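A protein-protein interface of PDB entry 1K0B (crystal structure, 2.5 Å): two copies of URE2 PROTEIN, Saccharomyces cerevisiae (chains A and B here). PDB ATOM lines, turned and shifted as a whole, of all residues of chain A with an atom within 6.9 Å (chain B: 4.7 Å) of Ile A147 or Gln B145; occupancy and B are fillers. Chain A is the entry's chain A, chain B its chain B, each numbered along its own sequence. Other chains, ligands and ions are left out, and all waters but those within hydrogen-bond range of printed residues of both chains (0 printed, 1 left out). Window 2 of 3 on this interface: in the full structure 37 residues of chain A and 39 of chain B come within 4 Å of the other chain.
Among the printed residues, pairs that only touch across the chains: Ser A149 with His B143 (2.8 Å), Ile A147 with Ile B147 (3.2 Å), Ile A147 with Gln B145 (3.96 Å) and Ser A149 with Ile B147 (3.96 Å).
Of the 6 printed residues of chain B, 4 touch a printed residue of chain A. Hydrophobic or aromatic side chains of chain B that line the printed part of chain A: His B143 and Ile B147. Of the 11 printed residues of chain A, 3 touch a printed residue of chain B. Hydrophobic or aromatic side chains of chain A that line the printed part of chain B: His A143 and Ile A147. Among the printed residues, no Asp or Glu carboxylate lies within 4 Å of a Lys or Arg side-chain nitrogen of the other chain.
NE2 of His A143 sits close to OG of Ser B149 (3.5 Å). NE2 of Gln B145 is in hydrogen-bond range of OG of Ser A149, 2.7 Å away.
ND1 of His A143 sits close to O of Gln A145. The backbone carbonyl oxygen of Gln B145 is in hydrogen-bond range of a ring nitrogen (ND1) of His B143 (3.4 Å).
Of the printed residues of chain B, His A143 touches Ser B149 (2.8 Å). Printed residues of chain B within 4 Å of Ile A147: Gln B145 (3.96 Å) and Ile B147 (3.2 Å). Of the printed residues of chain B, Ser A149 touches His B143, Gln B145 and Ile B147. Gln B145 touches just these residues of chain A: Ile A147 and Ser A149. Printed residues of chain A within 4 Å of Ile B147: Ile A147 (3.2 Å) and Ser A149 (3.96 Å). The nearest residue of chain B that does not touch Ile A147 is Ser B149 (4.4 Å). The nearest residue of chain A that does not touch Gln B145 is Ala A150 (5.5 Å).
His A143 touches Ser B149, and with the chains exchanged Ser A149 touches His B143. Ile A147 touches Gln B145, but with the chains exchanged Gln A145 does not touch Ile B147 (5.8 Å). Ser A149 touches Gln B145, but with the chains exchanged Gln A145 does not touch Ser B149 (4.7 Å). Ser A149 touches Ile B147, but with the chains exchanged Ile A147 does not touch Ser B149 (4.4 Å).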
ATOM      1  N   PHE A 139      12.851  -9.367 -10.400  1.00  0.00           N
ATOM      2  CA  PHE A 139      12.433  -8.069 -10.918  1.00  0.00           C
ATOM      3  C   PHE A 139      12.063  -8.069 -12.386  1.00  0.00           C
ATOM      4  O   PHE A 139      11.279  -7.229 -12.824  1.00  0.00           O
ATOM      5  CB  PHE A 139      13.510  -7.015 -10.643  1.00  0.00           C
ATOM      6  CG  PHE A 139      13.530  -6.552  -9.222  1.00  0.00           C
ATOM      7  CD1 PHE A 139      14.614  -6.826  -8.398  1.00  0.00           C
ATOM      8  CD2 PHE A 139      12.434  -5.871  -8.689  1.00  0.00           C
ATOM      9  CE1 PHE A 139      14.606  -6.427  -7.058  1.00  0.00           C
ATOM     10  CE2 PHE A 139      12.418  -5.470  -7.354  1.00  0.00           C
ATOM     11  CZ  PHE A 139      13.510  -5.750  -6.535  1.00  0.00           C
ATOM     12  N   ARG A 140      12.610  -9.016 -13.139  1.00  0.00           N
ATOM     13  CA  ARG A 140      12.306  -9.107 -14.556  1.00  0.00           C
ATOM     14  C   ARG A 140      11.042  -9.906 -14.855  1.00  0.00           C
ATOM     15  O   ARG A 140      10.322  -9.587 -15.802  1.00  0.00           O
ATOM     16  CB  ARG A 140      13.486  -9.724 -15.315  1.00  0.00           C
ATOM     17  CG  ARG A 140      13.209  -9.977 -16.794  1.00  0.00           C
ATOM     18  CD  ARG A 140      14.452  -9.721 -17.631  1.00  0.00           C
ATOM     19  NE  ARG A 140      14.329 -10.209 -19.006  1.00  0.00           N
ATOM     20  CZ  ARG A 140      15.280 -10.075 -19.930  1.00  0.00           C
ATOM     21  NH1 ARG A 140      15.099 -10.552 -21.159  1.00  0.00           N
ATOM     22  NH2 ARG A 140      16.415  -9.456 -19.626  1.00  0.00           N
ATOM     23  N   HIS A 143       8.263  -9.535 -10.136  1.00  0.00           N
ATOM     24  CA  HIS A 143       7.962  -8.473  -9.211  1.00  0.00           C
ATOM     25  C   HIS A 143       6.561  -7.950  -9.486  1.00  0.00           C
ATOM     26  O   HIS A 143       6.075  -8.024 -10.613  1.00  0.00           O
ATOM     27  CB  HIS A 143       8.989  -7.361  -9.304  1.00  0.00           C
ATOM     28  CG  HIS A 143       9.064  -6.541  -8.060  1.00  0.00           C
ATOM     29  ND1 HIS A 143       8.695  -5.213  -8.018  1.00  0.00           N
ATOM     30  CD2 HIS A 143       9.403  -6.878  -6.796  1.00  0.00           C
ATOM     31  CE1 HIS A 143       8.803  -4.771  -6.778  1.00  0.00           C
ATOM     32  NE2 HIS A 143       9.230  -5.761  -6.017  1.00  0.00           N
ATOM     33  N   GLN A 145       5.688  -5.175  -9.807  1.00  0.00           N
ATOM     34  CA  GLN A 145       5.798  -3.988 -10.641  1.00  0.00           C
ATOM     35  C   GLN A 145       7.026  -4.162 -11.537  1.00  0.00           C
ATOM     36  O   GLN A 145       7.923  -4.935 -11.205  1.00  0.00           O
ATOM     37  CB  GLN A 145       5.949  -2.767  -9.727  1.00  0.00           C
ATOM     38  CG  GLN A 145       5.578  -1.445 -10.353  1.00  0.00           C
ATOM     39  CD  GLN A 145       5.813  -0.275  -9.407  1.00  0.00           C
ATOM     40  OE1 GLN A 145       5.266  -0.235  -8.300  1.00  0.00           O
ATOM     41  NE2 GLN A 145       6.627   0.687  -9.841  1.00  0.00           N
ATOM     42  N   LYS A 146       7.062  -3.473 -12.675  1.00  0.00           N
ATOM     43  CA  LYS A 146       8.208  -3.580 -13.583  1.00  0.00           C
ATOM     44  C   LYS A 146       9.096  -2.353 -13.425  1.00  0.00           C
ATOM     45  O   LYS A 146       8.715  -1.255 -13.817  1.00  0.00           O
ATOM     46  CB  LYS A 146       7.749  -3.683 -15.044  1.00  0.00           C
ATOM     47  CG  LYS A 146       6.745  -4.796 -15.331  1.00  0.00           C
ATOM     48  CD  LYS A 146       7.273  -6.189 -14.948  1.00  0.00           C
ATOM     49  CE  LYS A 146       6.289  -7.296 -15.338  1.00  0.00           C
ATOM     50  NZ  LYS A 146       6.736  -8.646 -14.901  1.00  0.00           N
ATOM     51  N   ILE A 147      10.279  -2.541 -12.856  1.00  0.00           N
ATOM     52  CA  ILE A 147      11.210  -1.434 -12.634  1.00  0.00           C
ATOM     53  C   ILE A 147      12.591  -1.721 -13.228  1.00  0.00           C
ATOM     54  O   ILE A 147      13.346  -2.520 -12.696  1.00  0.00           O
ATOM     55  CB  ILE A 147      11.365  -1.169 -11.135  1.00  0.00           C
ATOM     56  CG1 ILE A 147       9.980  -1.084 -10.495  1.00  0.00           C
ATOM     57  CG2 ILE A 147      12.133   0.120 -10.915  1.00  0.00           C
ATOM     58  CD1 ILE A 147       9.976  -1.307  -9.011  1.00  0.00           C
ATOM     59  N   ALA A 148      12.919  -1.034 -14.314  1.00  0.00           N
ATOM     60  CA  ALA A 148      14.184  -1.236 -14.999  1.00  0.00           C
ATOM     61  C   ALA A 148      15.436  -0.963 -14.168  1.00  0.00           C
ATOM     62  O   ALA A 148      16.419  -1.696 -14.277  1.00  0.00           O
ATOM     63  CB  ALA A 148      14.208  -0.406 -16.281  1.00  0.00           C
ATOM     64  N   SER A 149      15.422   0.085 -13.351  1.00  0.00           N
ATOM     65  CA  SER A 149      16.595   0.385 -12.538  1.00  0.00           C
ATOM     66  C   SER A 149      16.943  -0.819 -11.667  1.00  0.00           C
ATOM     67  O   SER A 149      18.115  -1.120 -11.464  1.00  0.00           O
ATOM     68  CB  SER A 149      16.349   1.608 -11.652  1.00  0.00           C
ATOM     69  OG  SER A 149      15.347   1.354 -10.680  1.00  0.00           O
ATOM     70  N   ALA A 150      15.922  -1.503 -11.157  1.00  0.00           N
ATOM     71  CA  ALA A 150      16.139  -2.679 -10.323  1.00  0.00           C
ATOM     72  C   ALA A 150      16.661  -3.830 -11.180  1.00  0.00           C
ATOM     73  O   ALA A 150      17.604  -4.510 -10.793  1.00  0.00           O
ATOM     74  CB  ALA A 150      14.835  -3.090  -9.611  1.00  0.00           C
ATOM     75  N   VAL A 151      16.061  -4.056 -12.344  1.00  0.00           N
ATOM     76  CA  VAL A 151      16.536  -5.135 -13.202  1.00  0.00           C
ATOM     77  C   VAL A 151      17.987  -4.880 -13.606  1.00  0.00           C
ATOM     78  O   VAL A 151      18.824  -5.772 -13.533  1.00  0.00           O
ATOM     79  CB  VAL A 151      15.680  -5.287 -14.497  1.00  0.00           C
ATOM     80  CG1 VAL A 151      16.299  -6.347 -15.401  1.00  0.00           C
ATOM     81  CG2 VAL A 151      14.242  -5.692 -14.148  1.00  0.00           C
ATOM     82  N   GLU A 152      18.279  -3.656 -14.027  1.00  0.00           N
ATOM     83  CA  GLU A 152      19.626  -3.278 -14.454  1.00  0.00           C
ATOM     84  C   GLU A 152      20.656  -3.436 -13.331  1.00  0.00           C
ATOM     85  O   GLU A 152      21.790  -3.847 -13.576  1.00  0.00           O
ATOM     86  CB  GLU A 152      19.622  -1.834 -14.965  1.00  0.00           C
ATOM     87  CG  GLU A 152      20.964  -1.334 -15.481  1.00  0.00           C
ATOM     88  CD  GLU A 152      20.933   0.147 -15.824  1.00  0.00           C
ATOM     89  OE1 GLU A 152      21.966   0.682 -16.293  1.00  0.00           O
ATOM     90  OE2 GLU A 152      19.873   0.777 -15.619  1.00  0.00           O
ATOM     91  N   HIS B 143      19.597   3.547  -3.607  1.00  0.00           N
ATOM     92  CA  HIS B 143      19.163   3.386  -4.987  1.00  0.00           C
ATOM     93  C   HIS B 143      18.846   4.718  -5.679  1.00  0.00           C
ATOM     94  O   HIS B 143      18.456   5.699  -5.029  1.00  0.00           O
ATOM     95  CB  HIS B 143      17.948   2.467  -5.064  1.00  0.00           C
ATOM     96  CG  HIS B 143      17.773   1.837  -6.407  1.00  0.00           C
ATOM     97  ND1 HIS B 143      16.579   1.866  -7.097  1.00  0.00           N
ATOM     98  CD2 HIS B 143      18.650   1.175  -7.198  1.00  0.00           C
ATOM     99  CE1 HIS B 143      16.731   1.248  -8.256  1.00  0.00           C
ATOM    100  NE2 HIS B 143      17.978   0.821  -8.341  1.00  0.00           N
ATOM    101  N   SER B 144      19.004   4.733  -7.004  1.00  0.00           N
ATOM    102  CA  SER B 144      18.763   5.933  -7.810  1.00  0.00           C
ATOM    103  C   SER B 144      17.336   6.468  -7.724  1.00  0.00           C
ATOM    104  O   SER B 144      17.057   7.580  -8.171  1.00  0.00           O
ATOM    105  CB  SER B 144      19.127   5.669  -9.279  1.00  0.00           C
ATOM    106  OG  SER B 144      18.405   4.567  -9.805  1.00  0.00           O
ATOM    107  N   GLN B 145      16.431   5.675  -7.163  1.00  0.00           N
ATOM    108  CA  GLN B 145      15.042   6.095  -7.018  1.00  0.00           C
ATOM    109  C   GLN B 145      14.377   5.315  -5.900  1.00  0.00           C
ATOM    110  O   GLN B 145      14.917   4.319  -5.423  1.00  0.00           O
ATOM    111  CB  GLN B 145      14.272   5.905  -8.332  1.00  0.00           C
ATOM    112  CG  GLN B 145      14.038   4.464  -8.768  1.00  0.00           C
ATOM    113  CD  GLN B 145      13.368   4.382 -10.134  1.00  0.00           C
ATOM    114  OE1 GLN B 145      12.329   4.995 -10.365  1.00  0.00           O
ATOM    115  NE2 GLN B 145      13.966   3.624 -11.043  1.00  0.00           N
ATOM    116  N   LYS B 146      13.205   5.768  -5.476  1.00  0.00           N
ATOM    117  CA  LYS B 146      12.505   5.095  -4.395  1.00  0.00           C
ATOM    118  C   LYS B 146      11.545   4.011  -4.853  1.00  0.00           C
ATOM    119  O   LYS B 146      10.595   4.282  -5.587  1.00  0.00           O
ATOM    120  CB  LYS B 146      11.751   6.108  -3.528  1.00  0.00           C
ATOM    121  CG  LYS B 146      10.771   5.462  -2.553  1.00  0.00           C
ATOM    122  CD  LYS B 146      10.325   6.424  -1.460  1.00  0.00           C
ATOM    123  CE  LYS B 146       8.969   6.023  -0.868  1.00  0.00           C
ATOM    124  NZ  LYS B 146       7.850   6.218  -1.851  1.00  0.00           N
ATOM    125  N   ILE B 147      11.803   2.783  -4.408  1.00  0.00           N
ATOM    126  CA  ILE B 147      10.956   1.640  -4.729  1.00  0.00           C
ATOM    127  C   ILE B 147      10.515   1.011  -3.410  1.00  0.00           C
ATOM    128  O   ILE B 147      11.241   0.213  -2.817  1.00  0.00           O
ATOM    129  CB  ILE B 147      11.711   0.578  -5.528  1.00  0.00           C
ATOM    130  CG1 ILE B 147      12.418   1.220  -6.718  1.00  0.00           C
ATOM    131  CG2 ILE B 147      10.738  -0.490  -5.996  1.00  0.00           C
ATOM    132  CD1 ILE B 147      13.231   0.233  -7.524  1.00  0.00           C
ATOM    133  N   SER B 149       8.274  -1.261  -2.771  1.00  0.00           N
ATOM    134  CA  SER B 149       8.143  -2.706  -2.840  1.00  0.00           C
ATOM    135  C   SER B 149       9.488  -3.416  -2.722  1.00  0.00           C
ATOM    136  O   SER B 149       9.578  -4.481  -2.113  1.00  0.00           O
ATOM    137  CB  SER B 149       7.417  -3.114  -4.126  1.00  0.00           C
ATOM    138  OG  SER B 149       8.029  -2.568  -5.284  1.00  0.00           O
